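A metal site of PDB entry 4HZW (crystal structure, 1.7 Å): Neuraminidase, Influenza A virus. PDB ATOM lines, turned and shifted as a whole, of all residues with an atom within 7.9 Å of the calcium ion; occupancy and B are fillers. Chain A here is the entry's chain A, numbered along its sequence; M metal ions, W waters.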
ATOM      1  N   HIS A 195       7.957 -36.102 -24.670  1.00  0.00           N
ATOM      2  CA  HIS A 195       6.544 -36.167 -24.308  1.00  0.00           C
ATOM      3  C   HIS A 195       5.811 -35.055 -25.052  1.00  0.00           C
ATOM      4  O   HIS A 195       6.328 -33.950 -25.198  1.00  0.00           O
ATOM      5  CB  HIS A 195       6.361 -36.033 -22.783  1.00  0.00           C
ATOM      6  CG  HIS A 195       4.984 -36.407 -22.312  1.00  0.00           C
ATOM      7  ND1 HIS A 195       4.605 -37.712 -22.068  1.00  0.00           N
ATOM      8  CD2 HIS A 195       3.902 -35.643 -22.039  1.00  0.00           C
ATOM      9  CE1 HIS A 195       3.346 -37.732 -21.682  1.00  0.00           C
ATOM     10  NE2 HIS A 195       2.891 -36.493 -21.646  1.00  0.00           N
ATOM     11  N   CYS A 211       3.676 -27.612 -28.692  1.00  0.00           N
ATOM     12  CA  CYS A 211       2.858 -28.490 -27.852  1.00  0.00           C
ATOM     13  C   CYS A 211       3.198 -28.418 -26.368  1.00  0.00           C
ATOM     14  O   CYS A 211       3.866 -27.490 -25.909  1.00  0.00           O
ATOM     15  CB  CYS A 211       2.939 -29.923 -28.381  1.00  0.00           C
ATOM     16  SG  CYS A 211       2.888 -30.034 -30.187  1.00  0.00           S
ATOM     17  N   ARG A 212       2.694 -29.409 -25.627  1.00  0.00           N
ATOM     18  CA  ARG A 212       2.864 -29.502 -24.178  1.00  0.00           C
ATOM     19  C   ARG A 212       3.623 -30.783 -23.845  1.00  0.00           C
ATOM     20  O   ARG A 212       3.204 -31.876 -24.191  1.00  0.00           O
ATOM     21  CB  ARG A 212       1.483 -29.531 -23.512  1.00  0.00           C
ATOM     22  CG  ARG A 212       1.459 -29.918 -22.039  1.00  0.00           C
ATOM     23  CD  ARG A 212       0.008 -29.976 -21.553  1.00  0.00           C
ATOM     24  NE  ARG A 212      -0.136 -30.485 -20.186  1.00  0.00           N
ATOM     25  CZ  ARG A 212      -1.287 -30.457 -19.499  1.00  0.00           C
ATOM     26  NH1 ARG A 212      -2.367 -29.916 -20.041  1.00  0.00           N
ATOM     27  NH2 ARG A 212      -1.341 -30.942 -18.266  1.00  0.00           N
ATOM     28  N   ASP A 213       4.767 -30.633 -23.173  1.00  0.00           N
ATOM     29  CA  ASP A 213       5.489 -31.777 -22.636  1.00  0.00           C
ATOM     30  C   ASP A 213       5.087 -31.868 -21.176  1.00  0.00           C
ATOM     31  O   ASP A 213       5.384 -30.984 -20.402  1.00  0.00           O
ATOM     32  CB  ASP A 213       7.005 -31.549 -22.773  1.00  0.00           C
ATOM     33  CG  ASP A 213       7.823 -32.658 -22.113  1.00  0.00           C
ATOM     34  OD1 ASP A 213       7.451 -33.095 -21.006  1.00  0.00           O
ATOM     35  OD2 ASP A 213       8.841 -33.079 -22.697  1.00  0.00           O
ATOM     36  N   ASN A 214       4.370 -32.921 -20.802  1.00  0.00           N
ATOM     37  CA  ASN A 214       3.785 -33.015 -19.466  1.00  0.00           C
ATOM     38  C   ASN A 214       4.670 -33.738 -18.472  1.00  0.00           C
ATOM     39  O   ASN A 214       4.277 -33.956 -17.314  1.00  0.00           O
ATOM     40  CB  ASN A 214       2.425 -33.717 -19.537  1.00  0.00           C
ATOM     41  CG  ASN A 214       1.511 -33.347 -18.383  1.00  0.00           C
ATOM     42  OD1 ASN A 214       1.192 -32.176 -18.190  1.00  0.00           O
ATOM     43  ND2 ASN A 214       1.072 -34.345 -17.616  1.00  0.00           N
ATOM     44  N   TRP A 215       5.869 -34.104 -18.913  1.00  0.00           N
ATOM     45  CA  TRP A 215       6.710 -35.046 -18.179  1.00  0.00           C
ATOM     46  C   TRP A 215       7.988 -34.378 -17.664  1.00  0.00           C
ATOM     47  O   TRP A 215       8.081 -34.054 -16.481  1.00  0.00           O
ATOM     48  CB  TRP A 215       7.046 -36.231 -19.076  1.00  0.00           C
ATOM     49  CG  TRP A 215       7.877 -37.292 -18.424  1.00  0.00           C
ATOM     50  CD1 TRP A 215       8.110 -37.458 -17.092  1.00  0.00           C
ATOM     51  CD2 TRP A 215       8.603 -38.341 -19.090  1.00  0.00           C
ATOM     52  NE1 TRP A 215       8.937 -38.546 -16.892  1.00  0.00           N
ATOM     53  CE2 TRP A 215       9.262 -39.092 -18.106  1.00  0.00           C
ATOM     54  CE3 TRP A 215       8.763 -38.700 -20.440  1.00  0.00           C
ATOM     55  CZ2 TRP A 215      10.058 -40.198 -18.416  1.00  0.00           C
ATOM     56  CZ3 TRP A 215       9.559 -39.796 -20.740  1.00  0.00           C
ATOM     57  CH2 TRP A 215      10.194 -40.533 -19.731  1.00  0.00           C
ATOM     58  N   LYS A 216       8.945 -34.139 -18.548  1.00  0.00           N
ATOM     59  CA  LYS A 216      10.221 -33.540 -18.144  1.00  0.00           C
ATOM     60  C   LYS A 216      10.500 -32.150 -18.722  1.00  0.00           C
ATOM     61  O   LYS A 216      11.509 -31.536 -18.381  1.00  0.00           O
ATOM     62  CB  LYS A 216      11.383 -34.474 -18.527  1.00  0.00           C
ATOM     63  CG  LYS A 216      11.313 -35.854 -17.881  1.00  0.00           C
ATOM     64  CD  LYS A 216      12.427 -36.764 -18.389  1.00  0.00           C
ATOM     65  CE  LYS A 216      12.017 -37.566 -19.623  1.00  0.00           C
ATOM     66  NZ  LYS A 216      11.975 -36.759 -20.876  1.00  0.00           N
ATOM     67  N   GLY A 217       9.612 -31.626 -19.558  1.00  0.00           N
ATOM     68  CA  GLY A 217       9.914 -30.372 -20.240  1.00  0.00           C
ATOM     69  C   GLY A 217       9.138 -29.161 -19.775  1.00  0.00           C
ATOM     70  O   GLY A 217       7.920 -29.126 -19.863  1.00  0.00           O
ATOM     71  N   SER A 218       9.845 -28.141 -19.299  1.00  0.00           N
ATOM     72  CA  SER A 218       9.242 -26.843 -19.021  1.00  0.00           C
ATOM     73  C   SER A 218       9.289 -25.984 -20.286  1.00  0.00           C
ATOM     74  O   SER A 218       8.617 -24.947 -20.387  1.00  0.00           O
ATOM     75  CB  SER A 218       9.937 -26.126 -17.873  1.00  0.00           C
ATOM     76  OG  SER A 218      11.331 -25.979 -18.118  1.00  0.00           O
ATOM     77  N   ASN A 219      10.120 -26.412 -21.242  1.00  0.00           N
ATOM     78  CA  ASN A 219      10.123 -25.860 -22.591  1.00  0.00           C
ATOM     79  C   ASN A 219       9.137 -26.659 -23.446  1.00  0.00           C
ATOM     80  O   ASN A 219       8.834 -27.809 -23.136  1.00  0.00           O
ATOM     81  CB  ASN A 219      11.541 -25.882 -23.196  1.00  0.00           C
ATOM     82  CG  ASN A 219      12.212 -27.259 -23.086  1.00  0.00           C
ATOM     83  OD1 ASN A 219      11.842 -28.090 -22.256  1.00  0.00           O
ATOM     84  ND2 ASN A 219      13.233 -27.489 -23.921  1.00  0.00           N
ATOM     85  N   ARG A 220       8.633 -26.055 -24.523  1.00  0.00           N
ATOM     86  CA  ARG A 220       7.624 -26.706 -25.346  1.00  0.00           C
ATOM     87  C   ARG A 220       8.213 -27.440 -26.535  1.00  0.00           C
ATOM     88  O   ARG A 220       9.055 -26.890 -27.238  1.00  0.00           O
ATOM     89  CB  ARG A 220       6.603 -25.667 -25.847  1.00  0.00           C
ATOM     90  CG  ARG A 220       5.740 -25.101 -24.747  1.00  0.00           C
ATOM     91  CD  ARG A 220       4.510 -24.370 -25.309  1.00  0.00           C
ATOM     92  NE  ARG A 220       3.708 -23.820 -24.216  1.00  0.00           N
ATOM     93  CZ  ARG A 220       2.889 -24.530 -23.463  1.00  0.00           C
ATOM     94  NH1 ARG A 220       2.746 -25.837 -23.677  1.00  0.00           N
ATOM     95  NH2 ARG A 220       2.206 -23.943 -22.476  1.00  0.00           N
ATOM     96  N   PRO A 221       7.754 -28.671 -26.763  1.00  0.00           N
ATOM     97  CA  PRO A 221       8.129 -29.435 -27.970  1.00  0.00           C
ATOM     98  C   PRO A 221       7.492 -28.836 -29.202  1.00  0.00           C
ATOM     99  O   PRO A 221       6.434 -28.207 -29.084  1.00  0.00           O
ATOM    100  CB  PRO A 221       7.520 -30.829 -27.736  1.00  0.00           C
ATOM    101  CG  PRO A 221       6.835 -30.786 -26.417  1.00  0.00           C
ATOM    102  CD  PRO A 221       6.742 -29.369 -25.942  1.00  0.00           C
ATOM    103  N   TYR A 235      12.558 -28.887 -29.401  1.00  0.00           N
ATOM    104  CA  TYR A 235      11.919 -28.066 -28.359  1.00  0.00           C
ATOM    105  C   TYR A 235      12.245 -26.622 -28.682  1.00  0.00           C
ATOM    106  O   TYR A 235      13.267 -26.334 -29.304  1.00  0.00           O
ATOM    107  CB  TYR A 235      12.437 -28.435 -26.966  1.00  0.00           C
ATOM    108  CG  TYR A 235      11.859 -29.713 -26.389  1.00  0.00           C
ATOM    109  CD1 TYR A 235      12.334 -30.956 -26.780  1.00  0.00           C
ATOM    110  CD2 TYR A 235      10.841 -29.662 -25.435  1.00  0.00           C
ATOM    111  CE1 TYR A 235      11.807 -32.121 -26.255  1.00  0.00           C
ATOM    112  CE2 TYR A 235      10.306 -30.814 -24.913  1.00  0.00           C
ATOM    113  CZ  TYR A 235      10.790 -32.039 -25.322  1.00  0.00           C
ATOM    114  OH  TYR A 235      10.254 -33.191 -24.790  1.00  0.00           O
ATOM    115  N   ASP A 243       5.975 -23.154 -20.760  1.00  0.00           N
ATOM    116  CA  ASP A 243       5.007 -24.051 -20.150  1.00  0.00           C
ATOM    117  C   ASP A 243       4.672 -23.529 -18.742  1.00  0.00           C
ATOM    118  O   ASP A 243       5.296 -22.591 -18.263  1.00  0.00           O
ATOM    119  CB  ASP A 243       5.560 -25.471 -20.076  1.00  0.00           C
ATOM    120  CG  ASP A 243       4.472 -26.531 -19.972  1.00  0.00           C
ATOM    121  OD1 ASP A 243       3.268 -26.203 -19.952  1.00  0.00           O
ATOM    122  OD2 ASP A 243       4.829 -27.728 -19.909  1.00  0.00           O
ATOM    123  N   THR A 244       3.691 -24.146 -18.101  1.00  0.00           N
ATOM    124  CA  THR A 244       3.400 -23.881 -16.697  1.00  0.00           C
ATOM    125  C   THR A 244       3.137 -25.225 -16.044  1.00  0.00           C
ATOM    126  O   THR A 244       2.226 -25.932 -16.453  1.00  0.00           O
ATOM    127  CB  THR A 244       2.142 -23.009 -16.550  1.00  0.00           C
ATOM    128  OG1 THR A 244       2.301 -21.801 -17.304  1.00  0.00           O
ATOM    129  CG2 THR A 244       1.891 -22.652 -15.087  1.00  0.00           C
ATOM    130  N   PRO A 245       3.934 -25.599 -15.028  1.00  0.00           N
ATOM    131  CA  PRO A 245       4.991 -24.831 -14.372  1.00  0.00           C
ATOM    132  C   PRO A 245       6.257 -24.677 -15.222  1.00  0.00           C
ATOM    133  O   PRO A 245       6.405 -25.361 -16.238  1.00  0.00           O
ATOM    134  CB  PRO A 245       5.295 -25.649 -13.119  1.00  0.00           C
ATOM    135  CG  PRO A 245       4.943 -27.036 -13.472  1.00  0.00           C
ATOM    136  CD  PRO A 245       3.813 -26.964 -14.465  1.00  0.00           C
ATOM    137  N   ARG A 246       7.151 -23.802 -14.791  1.00  0.00           N
ATOM    138  CA  ARG A 246       8.414 -23.580 -15.470  1.00  0.00           C
ATOM    139  C   ARG A 246       9.344 -22.863 -14.513  1.00  0.00           C
ATOM    140  O   ARG A 246       8.897 -22.322 -13.501  1.00  0.00           O
ATOM    141  CB  ARG A 246       8.213 -22.734 -16.730  1.00  0.00           C
ATOM    142  CG  ARG A 246       7.685 -21.331 -16.438  1.00  0.00           C
ATOM    143  CD  ARG A 246       7.579 -20.478 -17.686  1.00  0.00           C
ATOM    144  NE  ARG A 246       7.157 -19.122 -17.358  1.00  0.00           N
ATOM    145  CZ  ARG A 246       5.888 -18.739 -17.272  1.00  0.00           C
ATOM    146  NH1 ARG A 246       5.601 -17.487 -16.951  1.00  0.00           N
ATOM    147  NH2 ARG A 246       4.900 -19.618 -17.489  1.00  0.00           N
ATOM    148  N   SER A 259      13.801 -29.636 -20.847  1.00  0.00           N
ATOM    149  CA  SER A 259      14.665 -28.934 -19.895  1.00  0.00           C
ATOM    150  C   SER A 259      15.087 -29.809 -18.706  1.00  0.00           C
ATOM    151  O   SER A 259      16.194 -29.657 -18.186  1.00  0.00           O
ATOM    152  CB  SER A 259      13.944 -27.686 -19.397  1.00  0.00           C
ATOM    153  OG  SER A 259      12.844 -28.054 -18.575  1.00  0.00           O
ATOM    154  N   VAL A 261      13.785 -29.487 -15.884  1.00  0.00           N
ATOM    155  CA  VAL A 261      13.595 -28.664 -14.687  1.00  0.00           C
ATOM    156  C   VAL A 261      12.146 -28.155 -14.647  1.00  0.00           C
ATOM    157  O   VAL A 261      11.630 -27.664 -15.652  1.00  0.00           O
ATOM    158  CB  VAL A 261      14.593 -27.474 -14.631  1.00  0.00           C
ATOM    159  CG1 VAL A 261      16.009 -27.992 -14.453  1.00  0.00           C
ATOM    160  CG2 VAL A 261      14.506 -26.636 -15.885  1.00  0.00           C
ATOM    161  N   ASN A 262      11.496 -28.311 -13.499  1.00  0.00           N
ATOM    162  CA  ASN A 262      10.073 -28.006 -13.376  1.00  0.00           C
ATOM    163  C   ASN A 262       9.281 -28.628 -14.508  1.00  0.00           C
ATOM    164  O   ASN A 262       8.389 -27.997 -15.081  1.00  0.00           O
ATOM    165  CB  ASN A 262       9.852 -26.493 -13.375  1.00  0.00           C
ATOM    166  CG  ASN A 262      10.460 -25.819 -12.173  1.00  0.00           C
ATOM    167  OD1 ASN A 262       9.963 -25.938 -11.053  1.00  0.00           O
ATOM    168  ND2 ASN A 262      11.539 -25.092 -12.404  1.00  0.00           N
ATOM    169  N   GLY A 263       9.599 -29.877 -14.822  1.00  0.00           N
ATOM    170  CA  GLY A 263       9.153 -30.486 -16.060  1.00  0.00           C
ATOM    171  C   GLY A 263       7.702 -30.899 -16.118  1.00  0.00           C
ATOM    172  O   GLY A 263       7.116 -30.883 -17.189  1.00  0.00           O
ATOM    173  N   GLY A 264       7.130 -31.309 -14.987  1.00  0.00           N
ATOM    174  CA  GLY A 264       5.749 -31.772 -14.987  1.00  0.00           C
ATOM    175  C   GLY A 264       4.899 -30.949 -14.036  1.00  0.00           C
ATOM    176  O   GLY A 264       5.417 -30.474 -13.014  1.00  0.00           O
ATOM    177  N   PRO A 265       3.601 -30.764 -14.342  1.00  0.00           N
ATOM    178  CA  PRO A 265       2.882 -31.237 -15.533  1.00  0.00           C
ATOM    179  C   PRO A 265       2.967 -30.247 -16.690  1.00  0.00           C
ATOM    180  O   PRO A 265       3.971 -30.230 -17.382  1.00  0.00           O
ATOM    181  CB  PRO A 265       1.419 -31.344 -15.048  1.00  0.00           C
ATOM    182  CG  PRO A 265       1.451 -31.065 -13.569  1.00  0.00           C
ATOM    183  CD  PRO A 265       2.674 -30.243 -13.328  1.00  0.00           C
ATOM    184  N   GLY A 266       1.939 -29.429 -16.899  1.00  0.00           N
ATOM    185  CA  GLY A 266       1.999 -28.467 -17.978  1.00  0.00           C
ATOM    186  C   GLY A 266       0.643 -27.807 -18.218  1.00  0.00           C
ATOM    187  O   GLY A 266      -0.286 -28.009 -17.453  1.00  0.00           O
ATOM    188  N   VAL A 267       0.570 -27.019 -19.272  1.00  0.00           N
ATOM    189  CA  VAL A 267      -0.688 -26.418 -19.714  1.00  0.00           C
ATOM    190  C   VAL A 267      -0.601 -26.292 -21.237  1.00  0.00           C
ATOM    191  O   VAL A 267       0.480 -26.133 -21.792  1.00  0.00           O
ATOM    192  CB  VAL A 267      -0.907 -25.026 -19.093  1.00  0.00           C
ATOM    193  CG1 VAL A 267       0.140 -24.038 -19.585  1.00  0.00           C
ATOM    194  CG2 VAL A 267      -2.303 -24.519 -19.410  1.00  0.00           C
HETATM  195 CA    CA M   1       5.796 -29.487 -18.641  1.00  0.00          CA
HETATM  196  O   HOH W   1       6.362 -27.904 -16.858  1.00  0.00           O
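The backbone carbonyl oxygen (O) of Pro 265 binds the calcium ion (2.3 Å). O of Asp 213 binds the calcium ion (2.3 Å). The side-chain carboxylate (OD2) of Asp 243 is bound to the calcium ion (2.4 Å). The calcium ion is bound by the backbone carbonyl oxygen (O) of Gly 263 (2.4 Å). Water W1 is bound to the calcium ion (2.5 Å). The calcium ion is bound by the backbone carbonyl oxygen (O) of Gly 217 (2.5 Å).
The side-chain carboxylate (OD1) of Asp 213 sits at hydrogen-bond distance from the backbone NH (N) of Gly 217 (3.0 Å). The side-chain carboxylate of Asp 213 sits at hydrogen-bond distance from the backbone NH of Trp 215, 2.8 Å away. N of Asp 243 lies close to O of Ser 218, at 3.2 Å. N of Val 267 sits at hydrogen-bond distance from OD1 of Asp 243 (2.9 Å). NH2 of Arg 220 is in salt-bridge range of OD1 of Asp 243 (3.6 Å). O of Asp 243 sits at hydrogen-bond distance from NH2 of Arg 246, 3.1 Å away. N of Gly 266 sits at hydrogen-bond distance from OD1 of Asn 214 (3.1 Å). The backbone carbonyl oxygen (O) of Gly 266 is in hydrogen-bond range of the guanidinium group (NH2) of Arg 212 (3.2 Å).
Merely in contact with the calcium ion: Gly 266 (3.99 Å). Of the 25 residues printed, 6 come within 4 Å of the calcium ion. Along chain A the residues within 4 Å of the calcium ion span positions 213 to 266. The nearest printed residue that does not touch the calcium ion is Asn 214 (4.1 Å).
Water W1 bridges O of Pro 245 (2.6 Å) and O of Asn 262 (2.7 Å).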
